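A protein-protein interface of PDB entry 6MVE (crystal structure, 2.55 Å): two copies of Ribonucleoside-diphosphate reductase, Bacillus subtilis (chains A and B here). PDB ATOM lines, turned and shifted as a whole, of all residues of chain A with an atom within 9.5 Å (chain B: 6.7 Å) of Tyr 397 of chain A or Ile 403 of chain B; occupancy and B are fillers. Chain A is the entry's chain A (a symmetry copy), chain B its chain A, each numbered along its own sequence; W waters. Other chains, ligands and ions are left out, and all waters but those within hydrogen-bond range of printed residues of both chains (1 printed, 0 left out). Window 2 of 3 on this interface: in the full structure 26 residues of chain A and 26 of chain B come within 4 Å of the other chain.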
ATOM      1  N   ASN A 180      18.978  12.274   6.957  1.00  0.00           N
ATOM      2  CA  ASN A 180      19.685  13.370   6.299  1.00  0.00           C
ATOM      3  C   ASN A 180      19.388  13.408   4.801  1.00  0.00           C
ATOM      4  O   ASN A 180      19.109  14.475   4.233  1.00  0.00           O
ATOM      5  CB  ASN A 180      21.192  13.235   6.508  1.00  0.00           C
ATOM      6  CG  ASN A 180      21.614  13.346   7.954  1.00  0.00           C
ATOM      7  OD1 ASN A 180      20.845  13.740   8.838  1.00  0.00           O
ATOM      8  ND2 ASN A 180      22.871  13.017   8.200  1.00  0.00           N
ATOM      9  N   ARG A 184      17.224  16.138   2.455  1.00  0.00           N
ATOM     10  CA  ARG A 184      17.854  16.850   1.359  1.00  0.00           C
ATOM     11  C   ARG A 184      17.131  16.603   0.035  1.00  0.00           C
ATOM     12  O   ARG A 184      17.059  17.509  -0.800  1.00  0.00           O
ATOM     13  CB  ARG A 184      19.331  16.454   1.290  1.00  0.00           C
ATOM     14  CG  ARG A 184      20.080  16.959   0.086  1.00  0.00           C
ATOM     15  CD  ARG A 184      20.180  18.441   0.120  1.00  0.00           C
ATOM     16  NE  ARG A 184      20.985  18.859   1.250  1.00  0.00           N
ATOM     17  CZ  ARG A 184      21.184  20.125   1.574  1.00  0.00           C
ATOM     18  NH1 ARG A 184      20.624  21.086   0.841  1.00  0.00           N
ATOM     19  NH2 ARG A 184      21.935  20.423   2.625  1.00  0.00           N
ATOM     20  N   TYR A 394      24.359  12.911   1.942  1.00  0.00           N
ATOM     21  CA  TYR A 394      24.332  14.188   2.626  1.00  0.00           C
ATOM     22  C   TYR A 394      24.453  13.868   4.104  1.00  0.00           C
ATOM     23  O   TYR A 394      23.547  13.270   4.689  1.00  0.00           O
ATOM     24  CB  TYR A 394      23.058  14.944   2.267  1.00  0.00           C
ATOM     25  CG  TYR A 394      22.959  15.169   0.768  1.00  0.00           C
ATOM     26  CD1 TYR A 394      23.674  16.183   0.155  1.00  0.00           C
ATOM     27  CD2 TYR A 394      22.175  14.338  -0.039  1.00  0.00           C
ATOM     28  CE1 TYR A 394      23.597  16.389  -1.231  1.00  0.00           C
ATOM     29  CE2 TYR A 394      22.089  14.534  -1.407  1.00  0.00           C
ATOM     30  CZ  TYR A 394      22.807  15.559  -2.004  1.00  0.00           C
ATOM     31  OH  TYR A 394      22.742  15.758  -3.367  1.00  0.00           O
ATOM     32  N   THR A 395      25.604  14.185   4.680  1.00  0.00           N
ATOM     33  CA  THR A 395      25.942  13.791   6.038  1.00  0.00           C
ATOM     34  C   THR A 395      25.446  14.846   7.021  1.00  0.00           C
ATOM     35  O   THR A 395      24.780  15.818   6.650  1.00  0.00           O
ATOM     36  CB  THR A 395      27.448  13.594   6.171  1.00  0.00           C
ATOM     37  OG1 THR A 395      28.104  14.810   5.793  1.00  0.00           O
ATOM     38  CG2 THR A 395      27.914  12.473   5.293  1.00  0.00           C
ATOM     39  N   ASP A 396      25.804  14.674   8.292  1.00  0.00           N
ATOM     40  CA  ASP A 396      25.453  15.627   9.336  1.00  0.00           C
ATOM     41  C   ASP A 396      25.890  17.037   8.976  1.00  0.00           C
ATOM     42  O   ASP A 396      26.748  17.238   8.105  1.00  0.00           O
ATOM     43  CB  ASP A 396      26.071  15.214  10.678  1.00  0.00           C
ATOM     44  CG  ASP A 396      25.253  14.155  11.415  1.00  0.00           C
ATOM     45  OD1 ASP A 396      24.294  13.585  10.837  1.00  0.00           O
ATOM     46  OD2 ASP A 396      25.577  13.897  12.600  1.00  0.00           O
ATOM     47  N   TYR A 397      25.295  18.016   9.659  1.00  0.00           N
ATOM     48  CA  TYR A 397      25.482  19.417   9.302  1.00  0.00           C
ATOM     49  C   TYR A 397      26.944  19.837   9.391  1.00  0.00           C
ATOM     50  O   TYR A 397      27.424  20.613   8.556  1.00  0.00           O
ATOM     51  CB  TYR A 397      24.613  20.295  10.199  1.00  0.00           C
ATOM     52  CG  TYR A 397      24.714  21.756   9.873  1.00  0.00           C
ATOM     53  CD1 TYR A 397      25.540  22.608  10.607  1.00  0.00           C
ATOM     54  CD2 TYR A 397      24.003  22.285   8.817  1.00  0.00           C
ATOM     55  CE1 TYR A 397      25.652  23.955  10.287  1.00  0.00           C
ATOM     56  CE2 TYR A 397      24.106  23.638   8.484  1.00  0.00           C
ATOM     57  CZ  TYR A 397      24.935  24.460   9.221  1.00  0.00           C
ATOM     58  OH  TYR A 397      25.018  25.787   8.891  1.00  0.00           O
ATOM     59  N   ASP A 398      27.670  19.353  10.396  1.00  0.00           N
ATOM     60  CA  ASP A 398      29.054  19.779  10.575  1.00  0.00           C
ATOM     61  C   ASP A 398      30.030  19.033   9.674  1.00  0.00           C
ATOM     62  O   ASP A 398      31.228  19.324   9.715  1.00  0.00           O
ATOM     63  CB  ASP A 398      29.488  19.642  12.047  1.00  0.00           C
ATOM     64  CG  ASP A 398      28.999  18.334  12.718  1.00  0.00           C
ATOM     65  OD1 ASP A 398      27.881  17.847  12.407  1.00  0.00           O
ATOM     66  OD2 ASP A 398      29.726  17.813  13.603  1.00  0.00           O
ATOM     67  N   GLU A 399      29.554  18.118   8.839  1.00  0.00           N
ATOM     68  CA  GLU A 399      30.430  17.246   8.078  1.00  0.00           C
ATOM     69  C   GLU A 399      30.279  17.472   6.581  1.00  0.00           C
ATOM     70  O   GLU A 399      29.243  17.941   6.092  1.00  0.00           O
ATOM     71  CB  GLU A 399      30.146  15.787   8.378  1.00  0.00           C
ATOM     72  CG  GLU A 399      30.257  15.415   9.816  1.00  0.00           C
ATOM     73  CD  GLU A 399      29.957  13.949  10.014  1.00  0.00           C
ATOM     74  OE1 GLU A 399      30.150  13.181   9.039  1.00  0.00           O
ATOM     75  OE2 GLU A 399      29.517  13.566  11.125  1.00  0.00           O
ATOM     76  N   GLU A 400      31.330  17.087   5.862  1.00  0.00           N
ATOM     77  CA  GLU A 400      31.340  17.194   4.413  1.00  0.00           C
ATOM     78  C   GLU A 400      30.358  16.205   3.807  1.00  0.00           C
ATOM     79  O   GLU A 400      30.252  15.063   4.256  1.00  0.00           O
ATOM     80  CB  GLU A 400      32.744  16.926   3.860  1.00  0.00           C
ATOM     81  CG  GLU A 400      33.799  17.981   4.196  1.00  0.00           C
ATOM     82  CD  GLU A 400      33.321  19.416   3.925  1.00  0.00           C
ATOM     83  OE1 GLU A 400      33.082  20.162   4.909  1.00  0.00           O
ATOM     84  OE2 GLU A 400      33.178  19.794   2.732  1.00  0.00           O
ATOM     85  N   ASP A 401      29.628  16.659   2.793  1.00  0.00           N
ATOM     86  CA  ASP A 401      28.766  15.771   2.039  1.00  0.00           C
ATOM     87  C   ASP A 401      29.586  15.032   0.989  1.00  0.00           C
ATOM     88  O   ASP A 401      30.677  15.452   0.609  1.00  0.00           O
ATOM     89  CB  ASP A 401      27.634  16.543   1.357  1.00  0.00           C
ATOM     90  CG  ASP A 401      26.760  17.295   2.343  1.00  0.00           C
ATOM     91  OD1 ASP A 401      26.278  18.402   1.998  1.00  0.00           O
ATOM     92  OD2 ASP A 401      26.564  16.780   3.468  1.00  0.00           O
ATOM     93  N   ARG B 184      15.121  23.790   6.069  1.00  0.00           N
ATOM     94  CA  ARG B 184      15.996  23.482   7.185  1.00  0.00           C
ATOM     95  C   ARG B 184      15.215  23.325   8.490  1.00  0.00           C
ATOM     96  O   ARG B 184      15.587  22.499   9.329  1.00  0.00           O
ATOM     97  CB  ARG B 184      17.073  24.565   7.287  1.00  0.00           C
ATOM     98  CG  ARG B 184      17.946  24.496   8.512  1.00  0.00           C
ATOM     99  CD  ARG B 184      18.776  23.263   8.490  1.00  0.00           C
ATOM    100  NE  ARG B 184      19.709  23.312   7.382  1.00  0.00           N
ATOM    101  CZ  ARG B 184      20.524  22.319   7.071  1.00  0.00           C
ATOM    102  NH1 ARG B 184      20.502  21.202   7.797  1.00  0.00           N
ATOM    103  NH2 ARG B 184      21.347  22.444   6.041  1.00  0.00           N
ATOM    104  N   GLN B 390      17.275  34.494  18.246  1.00  0.00           N
ATOM    105  CA  GLN B 390      17.595  35.223  17.027  1.00  0.00           C
ATOM    106  C   GLN B 390      17.603  34.261  15.849  1.00  0.00           C
ATOM    107  O   GLN B 390      18.260  33.217  15.897  1.00  0.00           O
ATOM    108  CB  GLN B 390      18.944  35.927  17.131  1.00  0.00           C
ATOM    109  CG  GLN B 390      19.143  36.744  18.396  1.00  0.00           C
ATOM    110  CD  GLN B 390      20.572  37.244  18.526  1.00  0.00           C
ATOM    111  OE1 GLN B 390      21.519  36.612  18.032  1.00  0.00           O
ATOM    112  NE2 GLN B 390      20.735  38.387  19.171  1.00  0.00           N
ATOM    113  N   VAL B 391      16.893  34.643  14.784  1.00  0.00           N
ATOM    114  CA  VAL B 391      16.676  33.774  13.637  1.00  0.00           C
ATOM    115  C   VAL B 391      17.976  33.565  12.874  1.00  0.00           C
ATOM    116  O   VAL B 391      18.809  34.478  12.750  1.00  0.00           O
ATOM    117  CB  VAL B 391      15.588  34.382  12.728  1.00  0.00           C
ATOM    118  CG1 VAL B 391      16.029  35.720  12.145  1.00  0.00           C
ATOM    119  CG2 VAL B 391      15.215  33.433  11.619  1.00  0.00           C
ATOM    120  N   SER B 392      18.153  32.360  12.356  1.00  0.00           N
ATOM    121  CA  SER B 392      19.252  32.077  11.457  1.00  0.00           C
ATOM    122  C   SER B 392      18.870  32.472  10.038  1.00  0.00           C
ATOM    123  O   SER B 392      17.726  32.824   9.742  1.00  0.00           O
ATOM    124  CB  SER B 392      19.607  30.593  11.494  1.00  0.00           C
ATOM    125  OG  SER B 392      19.933  30.186  12.797  1.00  0.00           O
ATOM    126  N   SER B 393      19.842  32.400   9.142  1.00  0.00           N
ATOM    127  CA  SER B 393      19.535  32.349   7.722  1.00  0.00           C
ATOM    128  C   SER B 393      20.349  31.211   7.128  1.00  0.00           C
ATOM    129  O   SER B 393      21.582  31.263   7.095  1.00  0.00           O
ATOM    130  CB  SER B 393      19.804  33.679   7.018  1.00  0.00           C
ATOM    131  OG  SER B 393      21.134  34.070   7.176  1.00  0.00           O
ATOM    132  N   TYR B 394      19.663  30.155   6.733  1.00  0.00           N
ATOM    133  CA  TYR B 394      20.296  29.041   6.057  1.00  0.00           C
ATOM    134  C   TYR B 394      20.275  29.388   4.580  1.00  0.00           C
ATOM    135  O   TYR B 394      19.206  29.455   3.970  1.00  0.00           O
ATOM    136  CB  TYR B 394      19.564  27.746   6.390  1.00  0.00           C
ATOM    137  CG  TYR B 394      19.555  27.491   7.888  1.00  0.00           C
ATOM    138  CD1 TYR B 394      20.667  26.969   8.524  1.00  0.00           C
ATOM    139  CD2 TYR B 394      18.441  27.812   8.670  1.00  0.00           C
ATOM    140  CE1 TYR B 394      20.670  26.742   9.910  1.00  0.00           C
ATOM    141  CE2 TYR B 394      18.432  27.591  10.037  1.00  0.00           C
ATOM    142  CZ  TYR B 394      19.552  27.060  10.658  1.00  0.00           C
ATOM    143  OH  TYR B 394      19.563  26.846  12.020  1.00  0.00           O
ATOM    144  N   GLU B 400      27.880  30.061   3.009  1.00  0.00           N
ATOM    145  CA  GLU B 400      27.907  29.964   4.459  1.00  0.00           C
ATOM    146  C   GLU B 400      26.548  30.323   5.034  1.00  0.00           C
ATOM    147  O   GLU B 400      25.894  31.262   4.576  1.00  0.00           O
ATOM    148  CB  GLU B 400      28.974  30.896   5.044  1.00  0.00           C
ATOM    149  CG  GLU B 400      30.423  30.514   4.740  1.00  0.00           C
ATOM    150  CD  GLU B 400      30.723  29.031   5.009  1.00  0.00           C
ATOM    151  OE1 GLU B 400      30.913  28.272   4.024  1.00  0.00           O
ATOM    152  OE2 GLU B 400      30.760  28.625   6.201  1.00  0.00           O
ATOM    153  N   ASP B 401      26.119  29.558   6.033  1.00  0.00           N
ATOM    154  CA  ASP B 401      24.910  29.890   6.761  1.00  0.00           C
ATOM    155  C   ASP B 401      25.224  30.933   7.825  1.00  0.00           C
ATOM    156  O   ASP B 401      26.368  31.114   8.235  1.00  0.00           O
ATOM    157  CB  ASP B 401      24.301  28.650   7.420  1.00  0.00           C
ATOM    158  CG  ASP B 401      23.946  27.567   6.418  1.00  0.00           C
ATOM    159  OD1 ASP B 401      24.076  26.365   6.759  1.00  0.00           O
ATOM    160  OD2 ASP B 401      23.546  27.922   5.286  1.00  0.00           O
ATOM    161  N   GLU B 402      24.190  31.619   8.271  1.00  0.00           N
ATOM    162  CA  GLU B 402      24.285  32.562   9.379  1.00  0.00           C
ATOM    163  C   GLU B 402      23.506  31.973  10.552  1.00  0.00           C
ATOM    164  O   GLU B 402      22.272  31.961  10.542  1.00  0.00           O
ATOM    165  CB  GLU B 402      23.743  33.921   8.959  1.00  0.00           C
ATOM    166  CG  GLU B 402      23.703  34.964  10.070  1.00  0.00           C
ATOM    167  CD  GLU B 402      23.608  36.397   9.538  1.00  0.00           C
ATOM    168  OE1 GLU B 402      23.768  36.610   8.296  1.00  0.00           O
ATOM    169  OE2 GLU B 402      23.377  37.302  10.378  1.00  0.00           O
ATOM    170  N   ILE B 403      24.225  31.466  11.547  1.00  0.00           N
ATOM    171  CA  ILE B 403      23.630  30.715  12.646  1.00  0.00           C
ATOM    172  C   ILE B 403      23.193  31.676  13.747  1.00  0.00           C
ATOM    173  O   ILE B 403      24.014  32.418  14.287  1.00  0.00           O
ATOM    174  CB  ILE B 403      24.623  29.682  13.190  1.00  0.00           C
ATOM    175  CG1 ILE B 403      25.099  28.785  12.056  1.00  0.00           C
ATOM    176  CG2 ILE B 403      23.982  28.864  14.293  1.00  0.00           C
ATOM    177  CD1 ILE B 403      24.002  27.946  11.430  1.00  0.00           C
ATOM    178  N   GLY B 404      21.912  31.648  14.097  1.00  0.00           N
ATOM    179  CA  GLY B 404      21.376  32.466  15.168  1.00  0.00           C
ATOM    180  C   GLY B 404      21.366  31.750  16.503  1.00  0.00           C
ATOM    181  O   GLY B 404      22.258  30.956  16.817  1.00  0.00           O
ATOM    182  N   LEU B 405      20.342  32.030  17.307  1.00  0.00           N
ATOM    183  CA  LEU B 405      20.179  31.406  18.617  1.00  0.00           C
ATOM    184  C   LEU B 405      18.774  30.826  18.712  1.00  0.00           C
ATOM    185  O   LEU B 405      17.795  31.577  18.778  1.00  0.00           O
ATOM    186  CB  LEU B 405      20.416  32.409  19.755  1.00  0.00           C
ATOM    187  CG  LEU B 405      21.784  33.087  19.898  1.00  0.00           C
ATOM    188  CD1 LEU B 405      21.696  34.319  20.767  1.00  0.00           C
ATOM    189  CD2 LEU B 405      22.831  32.121  20.451  1.00  0.00           C
ATOM    190  N   ARG B 446      23.412  17.464  17.431  1.00  0.00           N
ATOM    191  CA  ARG B 446      23.872  17.574  16.062  1.00  0.00           C
ATOM    192  C   ARG B 446      22.663  17.854  15.184  1.00  0.00           C
ATOM    193  O   ARG B 446      21.515  17.638  15.582  1.00  0.00           O
ATOM    194  CB  ARG B 446      24.588  16.296  15.613  1.00  0.00           C
ATOM    195  CG  ARG B 446      25.294  15.530  16.738  1.00  0.00           C
ATOM    196  CD  ARG B 446      26.393  16.368  17.378  1.00  0.00           C
ATOM    197  NE  ARG B 446      27.685  16.220  16.711  1.00  0.00           N
ATOM    198  CZ  ARG B 446      28.756  15.663  17.271  1.00  0.00           C
ATOM    199  NH1 ARG B 446      28.690  15.205  18.518  1.00  0.00           N
ATOM    200  NH2 ARG B 446      29.895  15.576  16.591  1.00  0.00           N
ATOM    201  N   ASN B 447      22.926  18.380  13.995  1.00  0.00           N
ATOM    202  CA  ASN B 447      21.887  18.648  13.010  1.00  0.00           C
ATOM    203  C   ASN B 447      20.887  19.703  13.487  1.00  0.00           C
ATOM    204  O   ASN B 447      19.766  19.782  12.978  1.00  0.00           O
ATOM    205  CB  ASN B 447      21.179  17.342  12.609  1.00  0.00           C
ATOM    206  CG  ASN B 447      22.116  16.365  11.906  1.00  0.00           C
ATOM    207  OD1 ASN B 447      23.045  16.775  11.200  1.00  0.00           O
ATOM    208  ND2 ASN B 447      21.882  15.077  12.094  1.00  0.00           N
ATOM    209  N   ALA B 448      21.283  20.532  14.455  1.00  0.00           N
ATOM    210  CA  ALA B 448      20.474  21.669  14.895  1.00  0.00           C
ATOM    211  C   ALA B 448      21.420  22.793  15.311  1.00  0.00           C
ATOM    212  O   ALA B 448      21.532  23.139  16.491  1.00  0.00           O
ATOM    213  CB  ALA B 448      19.545  21.258  16.037  1.00  0.00           C
ATOM    214  N   PRO B 449      22.111  23.405  14.348  1.00  0.00           N
ATOM    215  CA  PRO B 449      23.246  24.276  14.712  1.00  0.00           C
ATOM    216  C   PRO B 449      22.891  25.470  15.610  1.00  0.00           C
ATOM    217  O   PRO B 449      23.724  25.863  16.442  1.00  0.00           O
ATOM    218  CB  PRO B 449      23.792  24.725  13.348  1.00  0.00           C
ATOM    219  CG  PRO B 449      22.683  24.495  12.379  1.00  0.00           C
ATOM    220  CD  PRO B 449      21.871  23.359  12.897  1.00  0.00           C
ATOM    221  N   ALA B 450      21.694  26.061  15.489  1.00  0.00           N
ATOM    222  CA  ALA B 450      21.380  27.207  16.349  1.00  0.00           C
ATOM    223  C   ALA B 450      20.962  26.771  17.751  1.00  0.00           C
ATOM    224  O   ALA B 450      21.097  27.544  18.710  1.00  0.00           O
ATOM    225  CB  ALA B 450      20.285  28.073  15.719  1.00  0.00           C
ATOM    226  N   VAL B 451      20.427  25.560  17.884  1.00  0.00           N
ATOM    227  CA  VAL B 451      20.204  24.994  19.208  1.00  0.00           C
ATOM    228  C   VAL B 451      21.539  24.743  19.884  1.00  0.00           C
ATOM    229  O   VAL B 451      21.757  25.130  21.041  1.00  0.00           O
ATOM    230  CB  VAL B 451      19.369  23.701  19.111  1.00  0.00           C
ATOM    231  CG1 VAL B 451      19.367  22.984  20.416  1.00  0.00           C
ATOM    232  CG2 VAL B 451      17.938  23.995  18.649  1.00  0.00           C
ATOM    233  N   ARG B 453      24.450  26.121  19.255  1.00  0.00           N
ATOM    234  CA  ARG B 453      25.122  27.377  19.544  1.00  0.00           C
ATOM    235  C   ARG B 453      24.496  28.099  20.742  1.00  0.00           C
ATOM    236  O   ARG B 453      25.211  28.601  21.620  1.00  0.00           O
ATOM    237  CB  ARG B 453      25.105  28.247  18.296  1.00  0.00           C
ATOM    238  CG  ARG B 453      25.534  29.625  18.583  1.00  0.00           C
ATOM    239  CD  ARG B 453      25.829  30.411  17.359  1.00  0.00           C
ATOM    240  NE  ARG B 453      26.207  31.739  17.814  1.00  0.00           N
ATOM    241  CZ  ARG B 453      25.497  32.839  17.633  1.00  0.00           C
ATOM    242  NH1 ARG B 453      24.366  32.807  16.946  1.00  0.00           N
ATOM    243  NH2 ARG B 453      25.934  33.979  18.131  1.00  0.00           N
ATOM    244  N   ALA B 454      23.163  28.153  20.810  1.00  0.00           N
ATOM    245  CA  ALA B 454      22.520  28.858  21.914  1.00  0.00           C
ATOM    246  C   ALA B 454      22.749  28.165  23.254  1.00  0.00           C
ATOM    247  O   ALA B 454      22.771  28.830  24.295  1.00  0.00           O
ATOM    248  CB  ALA B 454      21.024  28.992  21.655  1.00  0.00           C
HETATM  249  O   HOH W   1      25.762  18.639  13.640  1.00  0.00           O
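The side-chain hydroxyl of Tyr 397 of chain A sits at hydrogen-bond distance from the side-chain carboxylate of Asp 401 of chain B (2.4 Å). The guanidinium group (NH2) of Arg 446 of chain B lies within salt-bridge range of the side-chain carboxylate (OD2) of Asp 398 of chain A (3.7 Å). OD1 of Asp 396 of chain A lies within hydrogen-bond range of ND2 of Asn 447 of chain B (3.1 Å). N of Tyr 397 of chain A lies within hydrogen-bond range of OD1 of Asn 447 of chain B, 3.0 Å away.
The backbone carbonyl oxygen (O) of Ile 403 of chain B lies within hydrogen-bond range of the guanidinium group (NH1) of Arg 453 of chain B (2.7 Å). The side-chain amide nitrogen (ND2) of Asn 180 of chain A sits at hydrogen-bond distance from the side-chain carboxylate (OD1) of Asp 396 of chain A.
Among the printed residues, merely in contact across the chains: Tyr 397 of chain A with Ile 403 of chain B (3.5 Å), Tyr 397 of chain A with Pro 449 of chain B (3.7 Å), Asn 180 of chain A with Asn 447 of chain B (3.7 Å), Tyr 397 of chain A with Arg 184 of chain B (3.8 Å) and Asp 396 of chain A with Arg 446 of chain B (3.98 Å).
Tyr 397 of chain A touches just these residues of chain B: Arg 184, Asp 401, Ile 403, Asn 447 and Pro 449. Ile 403 of chain B touches just one residue of chain A: Tyr 397 (3.5 Å). Asp 401 of chain B touches one residue of chain A. No residue of chain A comes within 4 Å of Gly 404 of chain B. Of chain A, only Tyr 397 (3.7 Å) comes within 4 Å of Pro 449 of chain B. Of the printed residues of chain A, Arg 184 of chain B touches Tyr 397 (3.8 Å). Printed residues of chain B within 4 Å of Asp 396 of chain A: Arg 446 (3.98 Å) and Asn 447 (3.1 Å). Printed residues of chain B within 4 Å of Asp 398 of chain A: Arg 446 (3.7 Å). Printed residues of chain A within 4 Å of Arg 446 of chain B: Asp 396 and Asp 398. Of the printed residues of chain A, Asn 447 of chain B touches Asn 180, Asp 396 and Tyr 397. Glu 402 of chain B touches none of the printed residues of chain A. Glu 400 of chain B touches none of the printed residues of chain A. The nearest residue of chain B that does not touch Tyr 397 of chain A is Tyr 394 of chain B (4.5 Å). The nearest printed residue of chain A that does not touch Arg 184 of chain B is Arg 184 of chain A (4.01 Å).
Of the 20 printed residues of chain B, 6 touch a printed residue of chain A. Of the 10 printed residues of chain A, 4 touch a printed residue of chain B. Hydrophobic or aromatic side chains of chain A that line the printed part of chain B: Tyr 397. Among the printed residues, Asp or Glu carboxylates within 4 Å of a Lys or Arg side-chain nitrogen of the other chain: Asp 398 of chain A with Arg 446 of chain B.
Positions printed for both chains: 184, 394, 400 and 401. Of the 9 pairs that touch across the chains among the printed residues, none has its exchanged pair printed and touching as well.
Water W1 bridges the side-chain carboxylate of Asp 398 of chain A (2.6 Å) and the backbone NH of Asn 447 of chain B (2.9 Å).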
